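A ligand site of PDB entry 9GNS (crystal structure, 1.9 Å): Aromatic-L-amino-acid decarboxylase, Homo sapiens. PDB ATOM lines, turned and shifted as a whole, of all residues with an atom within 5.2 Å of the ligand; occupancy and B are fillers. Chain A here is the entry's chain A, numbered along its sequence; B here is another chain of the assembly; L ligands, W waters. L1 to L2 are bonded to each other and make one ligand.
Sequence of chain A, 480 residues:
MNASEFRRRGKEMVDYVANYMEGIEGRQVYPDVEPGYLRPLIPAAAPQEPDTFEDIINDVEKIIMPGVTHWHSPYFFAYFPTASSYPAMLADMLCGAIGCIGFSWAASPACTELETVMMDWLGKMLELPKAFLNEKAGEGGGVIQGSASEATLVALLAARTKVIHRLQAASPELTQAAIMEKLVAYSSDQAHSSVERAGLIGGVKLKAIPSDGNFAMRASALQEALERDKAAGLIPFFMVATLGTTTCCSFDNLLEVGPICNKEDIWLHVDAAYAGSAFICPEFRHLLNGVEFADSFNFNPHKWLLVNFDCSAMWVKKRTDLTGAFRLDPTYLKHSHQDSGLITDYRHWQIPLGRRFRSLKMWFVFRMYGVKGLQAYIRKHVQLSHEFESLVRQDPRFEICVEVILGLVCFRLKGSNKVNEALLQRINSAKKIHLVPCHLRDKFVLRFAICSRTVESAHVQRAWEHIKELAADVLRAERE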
ATOM      1  N   TRP A  71       8.517 -24.562  28.753  1.00  0.00           N
ATOM      2  CA  TRP A  71       7.230 -23.859  28.690  1.00  0.00           C
ATOM      3  C   TRP A  71       6.196 -24.442  29.634  1.00  0.00           C
ATOM      4  O   TRP A  71       5.259 -23.743  30.055  1.00  0.00           O
ATOM      5  CB  TRP A  71       6.657 -23.923  27.275  1.00  0.00           C
ATOM      6  CG  TRP A  71       7.251 -22.949  26.312  1.00  0.00           C
ATOM      7  CD1 TRP A  71       8.506 -22.989  25.768  1.00  0.00           C
ATOM      8  CD2 TRP A  71       6.625 -21.778  25.790  1.00  0.00           C
ATOM      9  NE1 TRP A  71       8.684 -21.922  24.923  1.00  0.00           N
ATOM     10  CE2 TRP A  71       7.545 -21.152  24.925  1.00  0.00           C
ATOM     11  CE3 TRP A  71       5.365 -21.191  25.974  1.00  0.00           C
ATOM     12  CZ2 TRP A  71       7.249 -19.974  24.234  1.00  0.00           C
ATOM     13  CZ3 TRP A  71       5.072 -20.018  25.292  1.00  0.00           C
ATOM     14  CH2 TRP A  71       6.008 -19.422  24.429  1.00  0.00           C
ATOM     15  N   TYR A  79       5.558 -14.707  28.417  1.00  0.00           N
ATOM     16  CA  TYR A  79       4.717 -14.596  27.228  1.00  0.00           C
ATOM     17  C   TYR A  79       3.252 -14.874  27.544  1.00  0.00           C
ATOM     18  O   TYR A  79       2.624 -14.161  28.331  1.00  0.00           O
ATOM     19  CB  TYR A  79       5.233 -15.536  26.130  1.00  0.00           C
ATOM     20  CG  TYR A  79       6.744 -15.523  25.964  1.00  0.00           C
ATOM     21  CD1 TYR A  79       7.405 -14.391  25.485  1.00  0.00           C
ATOM     22  CD2 TYR A  79       7.507 -16.659  26.232  1.00  0.00           C
ATOM     23  CE1 TYR A  79       8.786 -14.376  25.321  1.00  0.00           C
ATOM     24  CE2 TYR A  79       8.900 -16.651  26.072  1.00  0.00           C
ATOM     25  CZ  TYR A  79       9.519 -15.501  25.616  1.00  0.00           C
ATOM     26  OH  TYR A  79      10.880 -15.479  25.425  1.00  0.00           O
ATOM     27  N   PHE A  80       2.697 -15.905  26.915  1.00  0.00           N
ATOM     28  CA  PHE A  80       1.388 -16.452  27.184  1.00  0.00           C
ATOM     29  C   PHE A  80       1.550 -17.969  27.229  1.00  0.00           C
ATOM     30  O   PHE A  80       2.517 -18.498  26.681  1.00  0.00           O
ATOM     31  CB  PHE A  80       0.377 -16.063  26.085  1.00  0.00           C
ATOM     32  CG  PHE A  80      -0.244 -14.698  26.261  1.00  0.00           C
ATOM     33  CD1 PHE A  80      -0.602 -14.226  27.510  1.00  0.00           C
ATOM     34  CD2 PHE A  80      -0.483 -13.894  25.158  1.00  0.00           C
ATOM     35  CE1 PHE A  80      -1.179 -12.971  27.661  1.00  0.00           C
ATOM     36  CE2 PHE A  80      -1.053 -12.636  25.297  1.00  0.00           C
ATOM     37  CZ  PHE A  80      -1.399 -12.170  26.551  1.00  0.00           C
ATOM     38  N   PRO A  81       0.634 -18.685  27.871  1.00  0.00           N
ATOM     39  CA  PRO A  81       0.727 -20.150  27.824  1.00  0.00           C
ATOM     40  C   PRO A  81       0.721 -20.658  26.388  1.00  0.00           C
ATOM     41  O   PRO A  81       0.131 -20.042  25.492  1.00  0.00           O
ATOM     42  CB  PRO A  81      -0.527 -20.618  28.586  1.00  0.00           C
ATOM     43  CG  PRO A  81      -1.488 -19.464  28.476  1.00  0.00           C
ATOM     44  CD  PRO A  81      -0.599 -18.234  28.535  1.00  0.00           C
ATOM     45  N   THR A  82       1.401 -21.776  26.176  1.00  0.00           N
ATOM     46  CA  THR A  82       1.111 -22.583  25.010  1.00  0.00           C
ATOM     47  C   THR A  82       0.561 -23.918  25.490  1.00  0.00           C
ATOM     48  O   THR A  82       0.810 -24.330  26.636  1.00  0.00           O
ATOM     49  CB  THR A  82       2.344 -22.778  24.098  1.00  0.00           C
ATOM     50  OG1 THR A  82       1.901 -23.243  22.807  1.00  0.00           O
ATOM     51  CG2 THR A  82       3.291 -23.815  24.672  1.00  0.00           C
ATOM     52  N   ALA A  83      -0.218 -24.562  24.639  1.00  0.00           N
ATOM     53  CA  ALA A  83      -1.016 -25.708  25.054  1.00  0.00           C
ATOM     54  C   ALA A  83      -0.180 -26.971  25.153  1.00  0.00           C
ATOM     55  O   ALA A  83       0.660 -27.259  24.289  1.00  0.00           O
ATOM     56  CB  ALA A  83      -2.171 -25.928  24.079  1.00  0.00           C
ATOM     57  N   GLY A 146      -2.614 -22.342  10.832  1.00  0.00           N
ATOM     58  CA  GLY A 146      -1.416 -22.754  11.553  1.00  0.00           C
ATOM     59  C   GLY A 146      -1.061 -21.859  12.724  1.00  0.00           C
ATOM     60  O   GLY A 146      -0.379 -22.305  13.651  1.00  0.00           O
ATOM     61  N   SER A 147      -1.530 -20.619  12.710  1.00  0.00           N
ATOM     62  CA  SER A 147      -1.147 -19.638  13.709  1.00  0.00           C
ATOM     63  C   SER A 147      -2.046 -18.420  13.557  1.00  0.00           C
ATOM     64  O   SER A 147      -2.628 -18.196  12.497  1.00  0.00           O
ATOM     65  CB  SER A 147       0.328 -19.266  13.569  1.00  0.00           C
ATOM     66  OG  SER A 147       0.536 -18.452  12.429  1.00  0.00           O
ATOM     67  N   ALA A 148      -2.155 -17.648  14.640  1.00  0.00           N
ATOM     68  CA  ALA A 148      -2.908 -16.403  14.567  1.00  0.00           C
ATOM     69  C   ALA A 148      -2.216 -15.404  13.648  1.00  0.00           C
ATOM     70  O   ALA A 148      -2.891 -14.581  13.014  1.00  0.00           O
ATOM     71  CB  ALA A 148      -3.104 -15.803  15.967  1.00  0.00           C
ATOM     72  N   SER A 149      -0.887 -15.443  13.574  1.00  0.00           N
ATOM     73  CA  SER A 149      -0.167 -14.568  12.651  1.00  0.00           C
ATOM     74  C   SER A 149      -0.590 -14.848  11.231  1.00  0.00           C
ATOM     75  O   SER A 149      -0.784 -13.927  10.434  1.00  0.00           O
ATOM     76  CB  SER A 149       1.340 -14.747  12.804  1.00  0.00           C
ATOM     77  OG  SER A 149       1.776 -14.462  14.118  1.00  0.00           O
ATOM     78  N   GLU A 150      -0.736 -16.131  10.891  1.00  0.00           N
ATOM     79  CA  GLU A 150      -1.185 -16.497   9.561  1.00  0.00           C
ATOM     80  C   GLU A 150      -2.656 -16.117   9.366  1.00  0.00           C
ATOM     81  O   GLU A 150      -3.046 -15.670   8.289  1.00  0.00           O
ATOM     82  CB  GLU A 150      -0.996 -17.998   9.328  1.00  0.00           C
ATOM     83  CG  GLU A 150       0.444 -18.382   9.051  1.00  0.00           C
ATOM     84  CD  GLU A 150       0.722 -19.855   9.344  1.00  0.00           C
ATOM     85  OE1 GLU A 150       0.646 -20.645   8.385  1.00  0.00           O
ATOM     86  OE2 GLU A 150       0.978 -20.222  10.513  1.00  0.00           O
ATOM     87  N   HIS A 192      -0.194  -7.021  18.276  1.00  0.00           N
ATOM     88  CA  HIS A 192       0.925  -7.940  18.131  1.00  0.00           C
ATOM     89  C   HIS A 192       1.675  -7.654  16.839  1.00  0.00           C
ATOM     90  O   HIS A 192       1.116  -7.152  15.861  1.00  0.00           O
ATOM     91  CB  HIS A 192       0.402  -9.385  18.147  1.00  0.00           C
ATOM     92  CG  HIS A 192       1.489 -10.427  18.154  1.00  0.00           C
ATOM     93  ND1 HIS A 192       1.870 -11.107  17.022  1.00  0.00           N
ATOM     94  CD2 HIS A 192       2.262 -10.895  19.161  1.00  0.00           C
ATOM     95  CE1 HIS A 192       2.836 -11.965  17.323  1.00  0.00           C
ATOM     96  NE2 HIS A 192       3.097 -11.844  18.610  1.00  0.00           N
ATOM     97  N   SER A 194       2.433  -9.477  14.585  1.00  0.00           N
ATOM     98  CA  SER A 194       1.875 -10.178  13.433  1.00  0.00           C
ATOM     99  C   SER A 194       1.066  -9.251  12.541  1.00  0.00           C
ATOM    100  O   SER A 194       0.940  -9.503  11.334  1.00  0.00           O
ATOM    101  CB  SER A 194       1.001 -11.349  13.891  1.00  0.00           C
ATOM    102  OG  SER A 194       0.074 -10.920  14.878  1.00  0.00           O
ATOM    103  N   THR A 242      -8.010  -6.029  18.799  1.00  0.00           N
ATOM    104  CA  THR A 242      -7.409  -7.061  19.634  1.00  0.00           C
ATOM    105  C   THR A 242      -8.186  -7.223  20.929  1.00  0.00           C
ATOM    106  O   THR A 242      -8.468  -6.242  21.623  1.00  0.00           O
ATOM    107  CB  THR A 242      -5.946  -6.736  19.938  1.00  0.00           C
ATOM    108  OG1 THR A 242      -5.222  -6.538  18.712  1.00  0.00           O
ATOM    109  CG2 THR A 242      -5.287  -7.858  20.745  1.00  0.00           C
ATOM    110  N   GLY A 244      -7.396  -8.978  24.277  1.00  0.00           N
ATOM    111  CA  GLY A 244      -6.298  -9.589  25.013  1.00  0.00           C
ATOM    112  C   GLY A 244      -4.936  -9.263  24.436  1.00  0.00           C
ATOM    113  O   GLY A 244      -4.250 -10.147  23.916  1.00  0.00           O
ATOM    114  N   THR A 245      -4.527  -7.996  24.532  1.00  0.00           N
ATOM    115  CA  THR A 245      -3.296  -7.562  23.897  1.00  0.00           C
ATOM    116  C   THR A 245      -2.098  -8.293  24.505  1.00  0.00           C
ATOM    117  O   THR A 245      -2.093  -8.672  25.679  1.00  0.00           O
ATOM    118  CB  THR A 245      -3.101  -6.051  24.041  1.00  0.00           C
ATOM    119  OG1 THR A 245      -3.153  -5.671  25.425  1.00  0.00           O
ATOM    120  CG2 THR A 245      -4.197  -5.310  23.270  1.00  0.00           C
ATOM    121  N   THR A 246      -1.074  -8.491  23.673  1.00  0.00           N
ATOM    122  CA  THR A 246       0.109  -9.233  24.106  1.00  0.00           C
ATOM    123  C   THR A 246       0.835  -8.515  25.232  1.00  0.00           C
ATOM    124  O   THR A 246       1.431  -9.170  26.106  1.00  0.00           O
ATOM    125  CB  THR A 246       1.047  -9.442  22.918  1.00  0.00           C
ATOM    126  OG1 THR A 246       0.274  -9.721  21.747  1.00  0.00           O
ATOM    127  CG2 THR A 246       1.997 -10.610  23.176  1.00  0.00           C
ATOM    128  N   ASP A 271      -8.720 -10.176  16.588  1.00  0.00           N
ATOM    129  CA  ASP A 271      -7.619 -11.021  17.035  1.00  0.00           C
ATOM    130  C   ASP A 271      -7.765 -11.209  18.538  1.00  0.00           C
ATOM    131  O   ASP A 271      -7.545 -10.277  19.312  1.00  0.00           O
ATOM    132  CB  ASP A 271      -6.294 -10.368  16.666  1.00  0.00           C
ATOM    133  CG  ASP A 271      -5.087 -11.001  17.359  1.00  0.00           C
ATOM    134  OD1 ASP A 271      -5.206 -12.067  17.990  1.00  0.00           O
ATOM    135  OD2 ASP A 271      -3.980 -10.427  17.230  1.00  0.00           O
ATOM    136  N   ALA A 273      -6.112 -13.944  20.123  1.00  0.00           N
ATOM    137  CA  ALA A 273      -5.218 -15.107  20.177  1.00  0.00           C
ATOM    138  C   ALA A 273      -5.207 -15.797  21.533  1.00  0.00           C
ATOM    139  O   ALA A 273      -5.412 -17.015  21.629  1.00  0.00           O
ATOM    140  CB  ALA A 273      -3.803 -14.677  19.793  1.00  0.00           C
ATOM    141  N   TYR A 274      -4.965 -15.032  22.596  1.00  0.00           N
ATOM    142  CA  TYR A 274      -4.875 -15.586  23.944  1.00  0.00           C
ATOM    143  C   TYR A 274      -6.229 -15.607  24.634  1.00  0.00           C
ATOM    144  O   TYR A 274      -6.700 -16.658  25.079  1.00  0.00           O
ATOM    145  CB  TYR A 274      -3.870 -14.780  24.783  1.00  0.00           C
ATOM    146  CG  TYR A 274      -4.007 -15.012  26.272  1.00  0.00           C
ATOM    147  CD1 TYR A 274      -3.664 -16.242  26.829  1.00  0.00           C
ATOM    148  CD2 TYR A 274      -4.495 -14.026  27.108  1.00  0.00           C
ATOM    149  CE1 TYR A 274      -3.784 -16.473  28.196  1.00  0.00           C
ATOM    150  CE2 TYR A 274      -4.625 -14.238  28.465  1.00  0.00           C
ATOM    151  CZ  TYR A 274      -4.267 -15.467  29.006  1.00  0.00           C
ATOM    152  OH  TYR A 274      -4.387 -15.681  30.360  1.00  0.00           O
ATOM    153  N   ASN A 300      -6.434 -18.637  19.462  1.00  0.00           N
ATOM    154  CA  ASN A 300      -5.551 -19.806  19.434  1.00  0.00           C
ATOM    155  C   ASN A 300      -5.931 -20.806  20.511  1.00  0.00           C
ATOM    156  O   ASN A 300      -5.585 -20.602  21.691  1.00  0.00           O
ATOM    157  CB  ASN A 300      -4.093 -19.368  19.637  1.00  0.00           C
ATOM    158  CG  ASN A 300      -3.523 -18.712  18.417  1.00  0.00           C
ATOM    159  OD1 ASN A 300      -4.028 -18.878  17.314  1.00  0.00           O
ATOM    160  ND2 ASN A 300      -2.466 -17.939  18.618  1.00  0.00           N
ATOM    161  N   HIS A 302      -4.232 -23.235  20.672  1.00  0.00           N
ATOM    162  CA  HIS A 302      -2.897 -23.680  21.057  1.00  0.00           C
ATOM    163  C   HIS A 302      -2.210 -22.738  22.045  1.00  0.00           C
ATOM    164  O   HIS A 302      -1.068 -23.024  22.439  1.00  0.00           O
ATOM    165  CB  HIS A 302      -2.019 -23.939  19.824  1.00  0.00           C
ATOM    166  CG  HIS A 302      -1.629 -22.731  19.030  1.00  0.00           C
ATOM    167  ND1 HIS A 302      -1.575 -22.747  17.653  1.00  0.00           N
ATOM    168  CD2 HIS A 302      -1.208 -21.493  19.398  1.00  0.00           C
ATOM    169  CE1 HIS A 302      -1.165 -21.571  17.210  1.00  0.00           C
ATOM    170  NE2 HIS A 302      -0.948 -20.789  18.254  1.00  0.00           N
ATOM    171  N   LYS A 303      -2.868 -21.668  22.482  1.00  0.00           N
ATOM    172  CA  LYS A 303      -2.381 -20.926  23.652  1.00  0.00           C
ATOM    173  C   LYS A 303      -3.080 -21.465  24.900  1.00  0.00           C
ATOM    174  O   LYS A 303      -2.467 -22.121  25.734  1.00  0.00           O
ATOM    175  CB  LYS A 303      -2.619 -19.413  23.497  1.00  0.00           C
ATOM    176  CG  LYS A 303      -1.590 -18.706  22.644  1.00  0.00           C
ATOM    177  CD  LYS A 303      -1.837 -17.196  22.666  1.00  0.00           C
ATOM    178  CE  LYS A 303      -0.740 -16.441  21.936  1.00  0.00           C
ATOM    179  NZ  LYS A 303      -0.480 -17.041  20.588  1.00  0.00           N
ATOM    180  N   PHE A 309       0.038 -26.754  19.902  1.00  0.00           N
ATOM    181  CA  PHE A 309       0.457 -26.131  18.648  1.00  0.00           C
ATOM    182  C   PHE A 309       0.795 -27.190  17.605  1.00  0.00           C
ATOM    183  O   PHE A 309       1.392 -28.216  17.920  1.00  0.00           O
ATOM    184  CB  PHE A 309       1.686 -25.248  18.953  1.00  0.00           C
ATOM    185  CG  PHE A 309       2.109 -24.355  17.818  1.00  0.00           C
ATOM    186  CD1 PHE A 309       2.876 -24.858  16.767  1.00  0.00           C
ATOM    187  CD2 PHE A 309       1.801 -23.012  17.826  1.00  0.00           C
ATOM    188  CE1 PHE A 309       3.294 -24.018  15.734  1.00  0.00           C
ATOM    189  CE2 PHE A 309       2.208 -22.166  16.788  1.00  0.00           C
ATOM    190  CZ  PHE A 309       2.955 -22.678  15.748  1.00  0.00           C
ATOM    191  N   ILE B 101       7.493 -23.132  21.703  1.00  0.00           N
ATOM    192  CA  ILE B 101       7.207 -22.313  20.527  1.00  0.00           C
ATOM    193  C   ILE B 101       8.483 -21.558  20.203  1.00  0.00           C
ATOM    194  O   ILE B 101       8.823 -20.593  20.903  1.00  0.00           O
ATOM    195  CB  ILE B 101       6.034 -21.357  20.767  1.00  0.00           C
ATOM    196  CG1 ILE B 101       4.847 -22.120  21.353  1.00  0.00           C
ATOM    197  CG2 ILE B 101       5.647 -20.659  19.449  1.00  0.00           C
ATOM    198  CD1 ILE B 101       4.374 -23.292  20.475  1.00  0.00           C
ATOM    199  N   PHE B 103       9.759 -19.102  18.546  1.00  0.00           N
ATOM    200  CA  PHE B 103       9.738 -17.837  17.814  1.00  0.00           C
ATOM    201  C   PHE B 103      10.950 -16.965  18.106  1.00  0.00           C
ATOM    202  O   PHE B 103      11.066 -15.881  17.544  1.00  0.00           O
ATOM    203  CB  PHE B 103       8.471 -17.049  18.153  1.00  0.00           C
ATOM    204  CG  PHE B 103       8.296 -16.814  19.633  1.00  0.00           C
ATOM    205  CD1 PHE B 103       8.992 -15.792  20.265  1.00  0.00           C
ATOM    206  CD2 PHE B 103       7.487 -17.640  20.385  1.00  0.00           C
ATOM    207  CE1 PHE B 103       8.852 -15.587  21.626  1.00  0.00           C
ATOM    208  CE2 PHE B 103       7.353 -17.432  21.734  1.00  0.00           C
ATOM    209  CZ  PHE B 103       8.024 -16.406  22.351  1.00  0.00           C
ATOM    210  N   LEU B 353       5.135 -16.540  12.874  1.00  0.00           N
ATOM    211  CA  LEU B 353       6.099 -16.239  13.934  1.00  0.00           C
ATOM    212  C   LEU B 353       6.388 -17.467  14.774  1.00  0.00           C
ATOM    213  O   LEU B 353       7.550 -17.771  15.061  1.00  0.00           O
ATOM    214  CB  LEU B 353       5.561 -15.135  14.858  1.00  0.00           C
ATOM    215  CG  LEU B 353       5.724 -13.645  14.568  1.00  0.00           C
ATOM    216  CD1 LEU B 353       7.160 -13.296  14.170  1.00  0.00           C
ATOM    217  CD2 LEU B 353       4.718 -13.222  13.521  1.00  0.00           C
ATOM    218  N   GLY B 354       5.337 -18.164  15.196  1.00  0.00           N
ATOM    219  CA  GLY B 354       5.513 -19.375  15.960  1.00  0.00           C
ATOM    220  C   GLY B 354       5.945 -20.538  15.104  1.00  0.00           C
ATOM    221  O   GLY B 354       5.736 -20.551  13.895  1.00  0.00           O
HETATM  222  N1  LIG L   1      -2.159 -11.887  18.456  1.00  0.00           N
HETATM  223  C1  LIG L   1      -1.803 -11.837  19.772  1.00  0.00           C
HETATM  224  C2  LIG L   1      -2.519 -10.908  20.698  1.00  0.00           C
HETATM  225  C3  LIG L   1      -0.773 -12.639  20.238  1.00  0.00           C
HETATM  226  O1  LIG L   1      -0.423 -12.579  21.561  1.00  0.00           O
HETATM  227  C4  LIG L   1      -0.111 -13.501  19.363  1.00  0.00           C
HETATM  228  C5  LIG L   1       1.147 -14.203  19.772  1.00  0.00           C
HETATM  229  C6  LIG L   1      -0.480 -13.526  18.028  1.00  0.00           C
HETATM  230  C7  LIG L   1      -1.507 -12.728  17.571  1.00  0.00           C
HETATM  231  C8  LIG L   1       0.226 -14.481  17.091  1.00  0.00           C
HETATM  232  O2  LIG L   1      -0.147 -15.796  17.450  1.00  0.00           O
HETATM  233  P1  LIG L   1       0.675 -17.030  16.822  1.00  0.00           P
HETATM  234  O3  LIG L   1      -0.225 -18.240  16.753  1.00  0.00           O
HETATM  235  O4  LIG L   1       1.090 -16.586  15.427  1.00  0.00           O
HETATM  236  O5  LIG L   1       1.900 -17.331  17.664  1.00  0.00           O
HETATM  237  N1  LG2 L   2       2.940 -14.289  21.037  1.00  0.00           N
HETATM  238  N2  LG2 L   2       1.529 -14.379  21.135  1.00  0.00           N
HETATM  239  C1  LG2 L   2       3.632 -14.439  22.340  1.00  0.00           C
HETATM  240  C2  LG2 L   2       4.410 -15.766  22.153  1.00  0.00           C
HETATM  241  C3  LG2 L   2       2.741 -14.318  23.584  1.00  0.00           C
HETATM  242  C4  LG2 L   2       3.542 -17.033  22.056  1.00  0.00           C
HETATM  243  C5  LG2 L   2       3.215 -17.537  20.806  1.00  0.00           C
HETATM  244  C6  LG2 L   2       2.432 -18.694  20.698  1.00  0.00           C
HETATM  245  C7  LG2 L   2       3.117 -17.702  23.206  1.00  0.00           C
HETATM  246  C8  LG2 L   2       2.333 -18.859  23.098  1.00  0.00           C
HETATM  247  C9  LG2 L   2       1.992 -19.351  21.834  1.00  0.00           C
HETATM  248  O1  LG2 L   2       1.184 -20.551  21.687  1.00  0.00           O
HETATM  249  O2  LG2 L   2       2.073 -19.225  19.407  1.00  0.00           O
HETATM  250  C10 LG2 L   2       4.745 -13.392  22.228  1.00  0.00           C
HETATM  251  O3  LG2 L   2       5.600 -13.298  23.115  1.00  0.00           O
HETATM  252  O4  LG2 L   2       4.767 -12.625  21.254  1.00  0.00           O
HETATM  253  O   HOH W   1       4.903  -9.786  21.411  1.00  0.00           O
HETATM  254  O   HOH W   2       4.106 -16.044  17.680  1.00  0.00           O
HETATM  255  O   HOH W   3       2.894 -17.514  13.956  1.00  0.00           O
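The backbone NH of Ser 149 is in hydrogen-bond range of an oxygen (O4) of LIG L1, at 2.9 Å.
An oxygen (O4) of LG2 L2 lies within hydrogen-bond range of a ring nitrogen (NE2) of His 192, at 3.2 Å.
O3 of LIG L1 lies within hydrogen-bond range of ND2 of Asn 300.
NZ of Lys 303 is in salt-bridge range of O5 of LIG L1, 3.8 Å away.
The backbone NH of Ala 148 sits at hydrogen-bond distance from an oxygen (O3) of LIG L1 (2.9 Å).
An oxygen (O3) of LIG L1 is in hydrogen-bond range of a ring nitrogen (NE2) of His 302, at 3.0 Å.
An oxygen (O1) of LG2 L2 lies within hydrogen-bond range of the side-chain hydroxyl (OG1) of Thr 82.
An oxygen (O1) of LIG L1 lies within hydrogen-bond range of the side-chain hydroxyl (OG1) of Thr 246 (2.9 Å).
O of His 302 lies within hydrogen-bond range of O1 of LG2 L2.
A nitrogen (N1) of LIG L1 sits at hydrogen-bond distance from the side-chain carboxylate (OD2) of Asp 271.
An oxygen (O4) of LIG L1 is in hydrogen-bond range of the side-chain hydroxyl of Ser 149, at 2.6 Å.
The side-chain carboxylate (OE2) of Glu 150 sits at hydrogen-bond distance from the side-chain hydroxyl (OG) of Ser 147 (2.6 Å).
The side-chain amide nitrogen (ND2) of Asn 300 lies close to the side-chain amino group (NZ) of Lys 303 (2.9 Å).
O of Lys 303 lies within hydrogen-bond range of N of Ala 83, 3.5 Å away.
A ring nitrogen (ND1) of His 192 sits at hydrogen-bond distance from the side-chain hydroxyl (OG) of Ser 194 (2.8 Å).
N of Asn 300 sits at hydrogen-bond distance from O of Ala 273 (2.9 Å).
N of Ala 273 sits at hydrogen-bond distance from OD1 of Asp 271.
O of His 302 sits at hydrogen-bond distance from N of Ala 83, at 2.8 Å.
The side-chain hydroxyl (OG1) of Thr 82 lies within hydrogen-bond range of the backbone carbonyl oxygen (O) of His 302, 3.0 Å away.
Residues that only touch the ligand: Tyr 79 (3.2 Å), Ser 147 (3.3 Å), Phe 103 of chain B (3.4 Å), Pro 81 (3.5 Å), Ala 273 (3.5 Å), Trp 71 (3.6 Å), Phe 80 (3.6 Å), Ser 194 (3.6 Å), Gly 244 (3.7 Å), Ile 101 of chain B (3.9 Å) and Phe 309 (3.9 Å).
Hydrophobic or aromatic side chains within 4 Å of the ligand: Trp 71, Tyr 79, Phe 80, Ala 148, His 192, Ala 273, His 302, Phe 309, Ile 101 of chain B and Phe 103 of chain B.
20 residues have an atom within 4 Å of the ligand: Trp 71, Tyr 79, Phe 80, Pro 81, Thr 82, Ser 147, Ala 148, Ser 149, His 192, Ser 194, Gly 244, Thr 246, Asp 271, Ala 273, Asn 300, His 302, Lys 303, Phe 309, Ile 101 of chain B and Phe 103 of chain B.
Water W3 lies within hydrogen-bond range of O4 of LIG L1, N of Leu 353 of chain B, N of Gly 354 of chain B, OG of Ser 147 and OG of Ser 149.
Water W2 bridges O5 of LIG L1 and N of Gly 354 of chain B.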
